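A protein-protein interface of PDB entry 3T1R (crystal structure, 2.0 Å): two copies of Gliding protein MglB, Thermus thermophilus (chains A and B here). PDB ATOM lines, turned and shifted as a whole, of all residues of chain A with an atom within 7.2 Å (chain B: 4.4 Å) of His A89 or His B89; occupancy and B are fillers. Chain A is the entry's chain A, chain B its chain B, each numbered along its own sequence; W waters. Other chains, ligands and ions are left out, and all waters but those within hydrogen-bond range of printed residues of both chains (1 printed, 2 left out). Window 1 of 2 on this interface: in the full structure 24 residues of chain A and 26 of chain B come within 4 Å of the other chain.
The backbone carbonyl oxygen of His A89 is in hydrogen-bond range of the backbone NH of Leu A96.
O of Glu A87 lies within hydrogen-bond range of N of Val A98 (3.0 Å).
The backbone NH (N) of His B89 lies within hydrogen-bond range of the backbone carbonyl oxygen (O) of Leu B96, 2.9 Å away.
The backbone carbonyl oxygen of Asn B68 lies close to the side-chain hydroxyl of Thr B72 (3.2 Å).
The side-chain amide nitrogen (ND2) of Asn B68 is in hydrogen-bond range of the side-chain carboxylate (OE1) of Glu B87 (3.2 Å).
The side-chain hydroxyl of Thr B72 sits at hydrogen-bond distance from the side-chain carboxylate of Glu B87 (3.2 Å).
Printed residues of chain B within 4 Å of Asn A68: Asn B68 and Thr B72.
Of the printed residues of chain B, Thr A72 touches Asn B68 and His B89.
Of the printed residues of chain B, Val A88 touches Glu B87 and Val B88.
Of chain B, only Phe B84, Glu B86, Glu B87 and His B89 come within 4 Å of His A89.
Printed residues of chain B within 4 Å of Gln A90: Phe B84 and Glu B86.
Val A98 touches none of the printed residues of chain B.
Phe A111 touches none of the printed residues of chain B.
Printed residues of chain A within 4 Å of His B89: Thr A72, Phe A84, Glu A86, Glu A87 and His A89.
The nearest printed residue of chain A that does not touch His B89 is Val A88 (5.1 Å).
The nearest printed residue of chain B that does not touch Glu A87 is Gln B90 (4.8 Å).
Asn A68 touches Thr B72, and with the chains exchanged Thr A72 touches Asn B68.
Thr A72 touches His B89, but with the chains exchanged His A89 does not touch Thr B72 (4.3 Å).
Glu A87 touches Val B88, and with the chains exchanged Val A88 touches Glu B87.
Val B88 touches its own counterpart, Val A88.
Of the 23 pairs that touch across the chains among the printed residues, 19 have their exchanged pair printed and touching as well.
N of Gln A90 lies within hydrogen-bond range of O of Glu B86 (2.8 Å).
OD1 of Asn B68 lies close to OD1 of Asn A68 (3.3 Å).
N of Gln A85 lies within hydrogen-bond range of O of Gln B90 (2.7 Å).
O of Glu A86 is in hydrogen-bond range of N of Gln B90 (2.7 Å).
The backbone NH (N) of Val A88 lies within hydrogen-bond range of the backbone carbonyl oxygen (O) of Val B88 (2.8 Å).
Among the printed residues, merely in contact across the chains: Asn A68 with Thr B72 (3.4 Å), Thr A72 with Asn B68 (3.0 Å), Thr A72 with His B89 (3.99 Å), Leu A75 with Leu B96 (3.6 Å), Phe A84 with His B89 (3.5 Å), Phe A84 with Gln B90 (3.6 Å), Phe A84 with Gly B91 (3.8 Å), Gln A85 with Gly B91 (3.8 Å), Glu A86 with His B89 (3.7 Å), Glu A87 with Val B88 (3.1 Å), Glu A87 with His B89 (3.4 Å), Val A88 with Glu B87 (3.2 Å), His A89 with Phe B84 (3.6 Å), His A89 with Glu B86 (3.7 Å), His A89 with Glu B87 (3.4 Å), His A89 with His B89 (3.97 Å), Gln A90 with Phe B84 (3.6 Å) and Gly A91 with Phe B84 (3.8 Å).
Hydrophobic or aromatic side chains of chain A within 4 Å of the printed part of chain B: Leu A75, Phe A84 and His A89.
Hydrophobic or aromatic side chains of chain B that line the printed part of chain A: Phe B84, His B89 and Leu B96.
Water W1 bridges OD1 of Asn A68 (2.7 Å) and OD1 of Asn B68 (3.2 Å).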
ATOM      1  N   ASN A  68      10.221  -5.426 -17.475  1.00  0.00           N
ATOM      2  CA  ASN A  68      10.530  -4.272 -18.269  1.00  0.00           C
ATOM      3  C   ASN A  68      10.661  -4.561 -19.765  1.00  0.00           C
ATOM      4  O   ASN A  68      10.165  -3.796 -20.556  1.00  0.00           O
ATOM      5  CB  ASN A  68      11.804  -3.584 -17.780  1.00  0.00           C
ATOM      6  CG  ASN A  68      12.087  -2.388 -18.568  1.00  0.00           C
ATOM      7  OD1 ASN A  68      11.336  -1.443 -18.473  1.00  0.00           O
ATOM      8  ND2 ASN A  68      13.126  -2.428 -19.435  1.00  0.00           N
ATOM      9  N   THR A  72       8.283  -2.603 -22.462  1.00  0.00           N
ATOM     10  CA  THR A  72       8.711  -1.520 -23.338  1.00  0.00           C
ATOM     11  C   THR A  72       8.357  -1.828 -24.776  1.00  0.00           C
ATOM     12  O   THR A  72       8.529  -0.966 -25.624  1.00  0.00           O
ATOM     13  CB  THR A  72      10.208  -1.194 -23.235  1.00  0.00           C
ATOM     14  OG1 THR A  72      10.967  -2.373 -23.566  1.00  0.00           O
ATOM     15  CG2 THR A  72      10.560  -0.647 -21.848  1.00  0.00           C
ATOM     16  N   LEU A  75       5.969   0.808 -26.524  1.00  0.00           N
ATOM     17  CA  LEU A  75       6.648   1.993 -26.905  1.00  0.00           C
ATOM     18  C   LEU A  75       7.468   1.753 -28.168  1.00  0.00           C
ATOM     19  O   LEU A  75       7.505   2.634 -29.053  1.00  0.00           O
ATOM     20  CB  LEU A  75       7.601   2.389 -25.791  1.00  0.00           C
ATOM     21  CG  LEU A  75       7.685   3.792 -25.249  1.00  0.00           C
ATOM     22  CD1 LEU A  75       8.920   3.864 -24.374  1.00  0.00           C
ATOM     23  CD2 LEU A  75       7.639   4.848 -26.359  1.00  0.00           C
ATOM     24  N   ALA A  76       8.202   0.634 -28.232  1.00  0.00           N
ATOM     25  CA  ALA A  76       8.938   0.299 -29.471  1.00  0.00           C
ATOM     26  C   ALA A  76       8.040   0.241 -30.718  1.00  0.00           C
ATOM     27  O   ALA A  76       8.457   0.700 -31.819  1.00  0.00           O
ATOM     28  CB  ALA A  76       9.712  -1.052 -29.352  1.00  0.00           C
ATOM     29  N   LEU A  79       7.160   3.436 -32.172  1.00  0.00           N
ATOM     30  CA  LEU A  79       8.245   3.903 -33.048  1.00  0.00           C
ATOM     31  C   LEU A  79       8.457   3.024 -34.297  1.00  0.00           C
ATOM     32  O   LEU A  79       9.368   3.246 -35.065  1.00  0.00           O
ATOM     33  CB  LEU A  79       9.541   4.059 -32.226  1.00  0.00           C
ATOM     34  CG  LEU A  79       9.226   4.852 -30.940  1.00  0.00           C
ATOM     35  CD1 LEU A  79      10.490   4.927 -29.975  1.00  0.00           C
ATOM     36  CD2 LEU A  79       8.822   6.276 -31.279  1.00  0.00           C
ATOM     37  N   PHE A  84      12.544  -3.181 -28.505  1.00  0.00           N
ATOM     38  CA  PHE A  84      13.880  -2.597 -28.478  1.00  0.00           C
ATOM     39  C   PHE A  84      14.936  -3.711 -28.544  1.00  0.00           C
ATOM     40  O   PHE A  84      14.664  -4.818 -28.124  1.00  0.00           O
ATOM     41  CB  PHE A  84      13.995  -1.743 -27.221  1.00  0.00           C
ATOM     42  CG  PHE A  84      13.170  -0.489 -27.309  1.00  0.00           C
ATOM     43  CD1 PHE A  84      13.491   0.497 -28.247  1.00  0.00           C
ATOM     44  CD2 PHE A  84      12.071  -0.284 -26.474  1.00  0.00           C
ATOM     45  CE1 PHE A  84      12.703   1.704 -28.369  1.00  0.00           C
ATOM     46  CE2 PHE A  84      11.295   0.938 -26.563  1.00  0.00           C
ATOM     47  CZ  PHE A  84      11.635   1.920 -27.546  1.00  0.00           C
ATOM     48  N   GLN A  85      16.095  -3.405 -29.128  1.00  0.00           N
ATOM     49  CA  GLN A  85      17.201  -4.336 -29.232  1.00  0.00           C
ATOM     50  C   GLN A  85      18.041  -4.219 -27.952  1.00  0.00           C
ATOM     51  O   GLN A  85      18.466  -5.232 -27.387  1.00  0.00           O
ATOM     52  CB  GLN A  85      18.032  -4.020 -30.468  1.00  0.00           C
ATOM     53  CG  GLN A  85      17.236  -4.127 -31.804  1.00  0.00           C
ATOM     54  CD  GLN A  85      16.957  -5.558 -32.203  1.00  0.00           C
ATOM     55  OE1 GLN A  85      15.928  -5.859 -32.814  1.00  0.00           O
ATOM     56  NE2 GLN A  85      17.867  -6.452 -31.855  1.00  0.00           N
ATOM     57  N   GLU A  86      18.261  -3.009 -27.458  1.00  0.00           N
ATOM     58  CA  GLU A  86      19.080  -2.850 -26.238  1.00  0.00           C
ATOM     59  C   GLU A  86      18.510  -1.703 -25.429  1.00  0.00           C
ATOM     60  O   GLU A  86      17.909  -0.807 -26.013  1.00  0.00           O
ATOM     61  CB  GLU A  86      20.613  -2.561 -26.542  1.00  0.00           C
ATOM     62  CG  GLU A  86      21.337  -3.721 -27.237  1.00  0.00           C
ATOM     63  CD  GLU A  86      21.282  -3.584 -28.778  1.00  0.00           C
ATOM     64  OE1 GLU A  86      21.031  -2.432 -29.178  1.00  0.00           O
ATOM     65  OE2 GLU A  86      21.389  -4.587 -29.566  1.00  0.00           O
ATOM     66  N   GLU A  87      18.757  -1.709 -24.109  1.00  0.00           N
ATOM     67  CA  GLU A  87      18.359  -0.588 -23.269  1.00  0.00           C
ATOM     68  C   GLU A  87      19.418  -0.373 -22.224  1.00  0.00           C
ATOM     69  O   GLU A  87      20.072  -1.369 -21.748  1.00  0.00           O
ATOM     70  CB  GLU A  87      17.060  -0.925 -22.488  1.00  0.00           C
ATOM     71  CG  GLU A  87      15.953  -1.443 -23.392  1.00  0.00           C
ATOM     72  CD  GLU A  87      14.629  -1.643 -22.649  1.00  0.00           C
ATOM     73  OE1 GLU A  87      13.699  -2.044 -23.344  1.00  0.00           O
ATOM     74  OE2 GLU A  87      14.537  -1.383 -21.392  1.00  0.00           O
ATOM     75  N   VAL A  88      19.591   0.899 -21.861  1.00  0.00           N
ATOM     76  CA  VAL A  88      20.556   1.268 -20.815  1.00  0.00           C
ATOM     77  C   VAL A  88      19.784   2.083 -19.819  1.00  0.00           C
ATOM     78  O   VAL A  88      19.119   3.013 -20.238  1.00  0.00           O
ATOM     79  CB  VAL A  88      21.727   2.139 -21.405  1.00  0.00           C
ATOM     80  CG1 VAL A  88      22.727   2.663 -20.299  1.00  0.00           C
ATOM     81  CG2 VAL A  88      22.565   1.233 -22.374  1.00  0.00           C
ATOM     82  N   HIS A  89      19.884   1.736 -18.534  1.00  0.00           N
ATOM     83  CA  HIS A  89      19.210   2.483 -17.479  1.00  0.00           C
ATOM     84  C   HIS A  89      20.331   2.912 -16.557  1.00  0.00           C
ATOM     85  O   HIS A  89      21.038   2.051 -16.114  1.00  0.00           O
ATOM     86  CB  HIS A  89      18.250   1.528 -16.691  1.00  0.00           C
ATOM     87  CG  HIS A  89      17.072   1.122 -17.520  1.00  0.00           C
ATOM     88  ND1 HIS A  89      17.127   0.073 -18.417  1.00  0.00           N
ATOM     89  CD2 HIS A  89      15.864   1.696 -17.683  1.00  0.00           C
ATOM     90  CE1 HIS A  89      15.967  -0.017 -19.050  1.00  0.00           C
ATOM     91  NE2 HIS A  89      15.180   0.948 -18.608  1.00  0.00           N
ATOM     92  N   GLN A  90      20.511   4.219 -16.359  1.00  0.00           N
ATOM     93  CA  GLN A  90      21.551   4.742 -15.508  1.00  0.00           C
ATOM     94  C   GLN A  90      20.938   5.434 -14.317  1.00  0.00           C
ATOM     95  O   GLN A  90      20.046   6.289 -14.481  1.00  0.00           O
ATOM     96  CB  GLN A  90      22.402   5.760 -16.280  1.00  0.00           C
ATOM     97  CG  GLN A  90      23.563   6.249 -15.468  1.00  0.00           C
ATOM     98  CD  GLN A  90      24.776   5.346 -15.612  1.00  0.00           C
ATOM     99  OE1 GLN A  90      25.222   5.074 -16.740  1.00  0.00           O
ATOM    100  NE2 GLN A  90      25.348   4.918 -14.468  1.00  0.00           N
ATOM    101  N   GLY A  91      21.396   5.057 -13.137  1.00  0.00           N
ATOM    102  CA  GLY A  91      21.048   5.774 -11.895  1.00  0.00           C
ATOM    103  C   GLY A  91      22.254   6.723 -11.695  1.00  0.00           C
ATOM    104  O   GLY A  91      23.073   6.912 -12.617  1.00  0.00           O
ATOM    105  N   MET A  94      24.567   3.402 -10.074  1.00  0.00           N
ATOM    106  CA  MET A  94      24.467   2.049 -10.652  1.00  0.00           C
ATOM    107  C   MET A  94      23.802   2.172 -12.034  1.00  0.00           C
ATOM    108  O   MET A  94      23.010   3.096 -12.256  1.00  0.00           O
ATOM    109  CB  MET A  94      23.624   1.152  -9.742  1.00  0.00           C
ATOM    110  CG  MET A  94      24.243   0.849  -8.354  1.00  0.00           C
ATOM    111  SD  MET A  94      25.801  -0.109  -8.454  1.00  0.00           S
ATOM    112  CE  MET A  94      25.391  -1.584  -9.253  1.00  0.00           C
ATOM    113  N   GLY A  95      24.139   1.277 -12.950  1.00  0.00           N
ATOM    114  CA  GLY A  95      23.450   1.202 -14.244  1.00  0.00           C
ATOM    115  C   GLY A  95      23.217  -0.234 -14.649  1.00  0.00           C
ATOM    116  O   GLY A  95      23.853  -1.142 -14.112  1.00  0.00           O
ATOM    117  N   LEU A  96      22.404  -0.401 -15.696  1.00  0.00           N
ATOM    118  CA  LEU A  96      22.121  -1.710 -16.228  1.00  0.00           C
ATOM    119  C   LEU A  96      22.135  -1.641 -17.752  1.00  0.00           C
ATOM    120  O   LEU A  96      21.661  -0.676 -18.370  1.00  0.00           O
ATOM    121  CB  LEU A  96      20.744  -2.173 -15.696  1.00  0.00           C
ATOM    122  CG  LEU A  96      19.889  -3.290 -16.300  1.00  0.00           C
ATOM    123  CD1 LEU A  96      20.089  -4.433 -15.404  1.00  0.00           C
ATOM    124  CD2 LEU A  96      18.468  -2.899 -16.184  1.00  0.00           C
ATOM    125  N   TYR A  97      22.697  -2.678 -18.359  1.00  0.00           N
ATOM    126  CA  TYR A  97      22.694  -2.727 -19.778  1.00  0.00           C
ATOM    127  C   TYR A  97      21.962  -4.056 -20.070  1.00  0.00           C
ATOM    128  O   TYR A  97      22.285  -5.054 -19.462  1.00  0.00           O
ATOM    129  CB  TYR A  97      24.154  -2.763 -20.329  1.00  0.00           C
ATOM    130  CG  TYR A  97      24.259  -3.130 -21.823  1.00  0.00           C
ATOM    131  CD1 TYR A  97      23.968  -2.182 -22.800  1.00  0.00           C
ATOM    132  CD2 TYR A  97      24.610  -4.450 -22.249  1.00  0.00           C
ATOM    133  CE1 TYR A  97      24.026  -2.479 -24.192  1.00  0.00           C
ATOM    134  CE2 TYR A  97      24.668  -4.751 -23.640  1.00  0.00           C
ATOM    135  CZ  TYR A  97      24.413  -3.760 -24.586  1.00  0.00           C
ATOM    136  OH  TYR A  97      24.446  -4.048 -25.942  1.00  0.00           O
ATOM    137  N   VAL A  98      21.040  -4.066 -21.026  1.00  0.00           N
ATOM    138  CA  VAL A  98      20.287  -5.281 -21.366  1.00  0.00           C
ATOM    139  C   VAL A  98      20.307  -5.426 -22.859  1.00  0.00           C
ATOM    140  O   VAL A  98      20.052  -4.441 -23.575  1.00  0.00           O
ATOM    141  CB  VAL A  98      18.796  -5.200 -20.935  1.00  0.00           C
ATOM    142  CG1 VAL A  98      18.087  -6.574 -21.306  1.00  0.00           C
ATOM    143  CG2 VAL A  98      18.701  -4.928 -19.443  1.00  0.00           C
ATOM    144  N   LEU A 109      23.955  -6.745 -17.751  1.00  0.00           N
ATOM    145  CA  LEU A 109      25.171  -6.361 -17.070  1.00  0.00           C
ATOM    146  C   LEU A 109      24.783  -5.255 -16.075  1.00  0.00           C
ATOM    147  O   LEU A 109      24.150  -4.240 -16.442  1.00  0.00           O
ATOM    148  CB  LEU A 109      26.204  -5.791 -18.087  1.00  0.00           C
ATOM    149  CG  LEU A 109      26.771  -6.797 -19.086  1.00  0.00           C
ATOM    150  CD1 LEU A 109      27.664  -6.135 -20.140  1.00  0.00           C
ATOM    151  CD2 LEU A 109      27.538  -7.950 -18.416  1.00  0.00           C
ATOM    152  N   PHE A 111      26.381  -2.410 -13.556  1.00  0.00           N
ATOM    153  CA  PHE A 111      27.711  -1.788 -13.428  1.00  0.00           C
ATOM    154  C   PHE A 111      27.657  -0.529 -12.512  1.00  0.00           C
ATOM    155  O   PHE A 111      26.556   0.001 -12.256  1.00  0.00           O
ATOM    156  CB  PHE A 111      28.265  -1.464 -14.802  1.00  0.00           C
ATOM    157  CG  PHE A 111      27.362  -0.606 -15.649  1.00  0.00           C
ATOM    158  CD1 PHE A 111      27.489   0.787 -15.629  1.00  0.00           C
ATOM    159  CD2 PHE A 111      26.369  -1.208 -16.490  1.00  0.00           C
ATOM    160  CE1 PHE A 111      26.653   1.600 -16.373  1.00  0.00           C
ATOM    161  CE2 PHE A 111      25.536  -0.423 -17.244  1.00  0.00           C
ATOM    162  CZ  PHE A 111      25.668   0.999 -17.196  1.00  0.00           C
ATOM    163  N   ASN B  68       6.434   3.625 -18.247  1.00  0.00           N
ATOM    164  CA  ASN B  68       7.768   2.996 -18.084  1.00  0.00           C
ATOM    165  C   ASN B  68       8.563   3.641 -16.952  1.00  0.00           C
ATOM    166  O   ASN B  68       9.206   2.948 -16.140  1.00  0.00           O
ATOM    167  CB  ASN B  68       8.546   3.051 -19.421  1.00  0.00           C
ATOM    168  CG  ASN B  68       9.980   2.539 -19.315  1.00  0.00           C
ATOM    169  OD1 ASN B  68      10.229   1.401 -19.647  1.00  0.00           O
ATOM    170  ND2 ASN B  68      10.940   3.397 -18.913  1.00  0.00           N
ATOM    171  N   THR B  72       9.809   1.331 -13.847  1.00  0.00           N
ATOM    172  CA  THR B  72      11.221   0.917 -13.604  1.00  0.00           C
ATOM    173  C   THR B  72      11.741   1.368 -12.223  1.00  0.00           C
ATOM    174  O   THR B  72      12.867   1.069 -11.862  1.00  0.00           O
ATOM    175  CB  THR B  72      12.168   1.434 -14.745  1.00  0.00           C
ATOM    176  OG1 THR B  72      12.121   2.859 -14.796  1.00  0.00           O
ATOM    177  CG2 THR B  72      11.707   0.967 -16.056  1.00  0.00           C
ATOM    178  N   PHE B  84      15.788   5.606 -11.911  1.00  0.00           N
ATOM    179  CA  PHE B  84      16.794   5.880 -12.942  1.00  0.00           C
ATOM    180  C   PHE B  84      16.823   7.379 -13.294  1.00  0.00           C
ATOM    181  O   PHE B  84      15.792   8.045 -13.160  1.00  0.00           O
ATOM    182  CB  PHE B  84      16.595   4.931 -14.151  1.00  0.00           C
ATOM    183  CG  PHE B  84      16.902   3.476 -13.806  1.00  0.00           C
ATOM    184  CD1 PHE B  84      18.183   3.115 -13.445  1.00  0.00           C
ATOM    185  CD2 PHE B  84      15.898   2.511 -13.778  1.00  0.00           C
ATOM    186  CE1 PHE B  84      18.515   1.783 -13.086  1.00  0.00           C
ATOM    187  CE2 PHE B  84      16.202   1.173 -13.415  1.00  0.00           C
ATOM    188  CZ  PHE B  84      17.505   0.830 -13.057  1.00  0.00           C
ATOM    189  N   GLU B  86      18.697   8.540 -16.281  1.00  0.00           N
ATOM    190  CA  GLU B  86      18.606   8.537 -17.730  1.00  0.00           C
ATOM    191  C   GLU B  86      18.424   7.145 -18.257  1.00  0.00           C
ATOM    192  O   GLU B  86      18.946   6.162 -17.665  1.00  0.00           O
ATOM    193  CB  GLU B  86      19.933   9.056 -18.326  1.00  0.00           C
ATOM    194  CG  GLU B  86      20.182  10.557 -18.014  1.00  0.00           C
ATOM    195  CD  GLU B  86      21.130  10.769 -16.823  1.00  0.00           C
ATOM    196  OE1 GLU B  86      21.124  11.885 -16.168  1.00  0.00           O
ATOM    197  OE2 GLU B  86      21.872   9.783 -16.554  1.00  0.00           O
ATOM    198  N   GLU B  87      17.747   7.067 -19.408  1.00  0.00           N
ATOM    199  CA  GLU B  87      17.549   5.765 -20.087  1.00  0.00           C
ATOM    200  C   GLU B  87      17.656   5.935 -21.609  1.00  0.00           C
ATOM    201  O   GLU B  87      17.190   6.958 -22.158  1.00  0.00           O
ATOM    202  CB  GLU B  87      16.121   5.287 -19.735  1.00  0.00           C
ATOM    203  CG  GLU B  87      15.955   5.050 -18.150  1.00  0.00           C
ATOM    204  CD  GLU B  87      14.477   4.862 -17.741  1.00  0.00           C
ATOM    205  OE1 GLU B  87      13.595   5.077 -18.586  1.00  0.00           O
ATOM    206  OE2 GLU B  87      14.176   4.493 -16.607  1.00  0.00           O
ATOM    207  N   VAL B  88      18.268   4.939 -22.265  1.00  0.00           N
ATOM    208  CA  VAL B  88      18.279   4.863 -23.689  1.00  0.00           C
ATOM    209  C   VAL B  88      17.627   3.548 -24.103  1.00  0.00           C
ATOM    210  O   VAL B  88      17.980   2.499 -23.536  1.00  0.00           O
ATOM    211  CB  VAL B  88      19.767   4.886 -24.199  1.00  0.00           C
ATOM    212  CG1 VAL B  88      19.848   4.494 -25.695  1.00  0.00           C
ATOM    213  CG2 VAL B  88      20.370   6.271 -23.900  1.00  0.00           C
ATOM    214  N   HIS B  89      16.688   3.618 -25.028  1.00  0.00           N
ATOM    215  CA  HIS B  89      16.050   2.406 -25.569  1.00  0.00           C
ATOM    216  C   HIS B  89      16.439   2.444 -27.013  1.00  0.00           C
ATOM    217  O   HIS B  89      16.127   3.414 -27.713  1.00  0.00           O
ATOM    218  CB  HIS B  89      14.526   2.485 -25.428  1.00  0.00           C
ATOM    219  CG  HIS B  89      14.072   2.536 -24.003  1.00  0.00           C
ATOM    220  ND1 HIS B  89      13.995   3.714 -23.281  1.00  0.00           N
ATOM    221  CD2 HIS B  89      13.728   1.549 -23.147  1.00  0.00           C
ATOM    222  CE1 HIS B  89      13.588   3.448 -22.053  1.00  0.00           C
ATOM    223  NE2 HIS B  89      13.408   2.143 -21.950  1.00  0.00           N
ATOM    224  N   GLN B  90      17.138   1.403 -27.450  1.00  0.00           N
ATOM    225  CA  GLN B  90      17.649   1.380 -28.763  1.00  0.00           C
ATOM    226  C   GLN B  90      16.972   0.283 -29.618  1.00  0.00           C
ATOM    227  O   GLN B  90      17.046  -0.906 -29.299  1.00  0.00           O
ATOM    228  CB  GLN B  90      19.152   1.089 -28.590  1.00  0.00           C
ATOM    229  CG  GLN B  90      19.883   0.985 -29.860  1.00  0.00           C
ATOM    230  CD  GLN B  90      20.131   2.365 -30.427  1.00  0.00           C
ATOM    231  OE1 GLN B  90      20.735   3.214 -29.739  1.00  0.00           O
ATOM    232  NE2 GLN B  90      19.673   2.598 -31.700  1.00  0.00           N
ATOM    233  N   GLY B  91      16.326   0.689 -30.708  1.00  0.00           N
ATOM    234  CA  GLY B  91      15.820  -0.266 -31.698  1.00  0.00           C
ATOM    235  C   GLY B  91      16.829  -0.512 -32.797  1.00  0.00           C
ATOM    236  O   GLY B  91      17.981  -0.082 -32.710  1.00  0.00           O
ATOM    237  N   GLY B  95      15.409   5.206 -31.850  1.00  0.00           N
ATOM    238  CA  GLY B  95      15.865   5.154 -30.465  1.00  0.00           C
ATOM    239  C   GLY B  95      15.135   6.254 -29.718  1.00  0.00           C
ATOM    240  O   GLY B  95      14.585   7.189 -30.356  1.00  0.00           O
ATOM    241  N   LEU B  96      15.243   6.165 -28.387  1.00  0.00           N
ATOM    242  CA  LEU B  96      14.652   7.062 -27.474  1.00  0.00           C
ATOM    243  C   LEU B  96      15.617   7.327 -26.359  1.00  0.00           C
ATOM    244  O   LEU B  96      16.219   6.386 -25.859  1.00  0.00           O
ATOM    245  CB  LEU B  96      13.503   6.336 -26.823  1.00  0.00           C
ATOM    246  CG  LEU B  96      12.361   7.093 -26.263  1.00  0.00           C
ATOM    247  CD1 LEU B  96      11.766   7.815 -27.454  1.00  0.00           C
ATOM    248  CD2 LEU B  96      11.477   5.948 -25.886  1.00  0.00           C
HETATM  249  O   HOH W   1       8.806  -0.794 -17.786  1.00  0.00           O
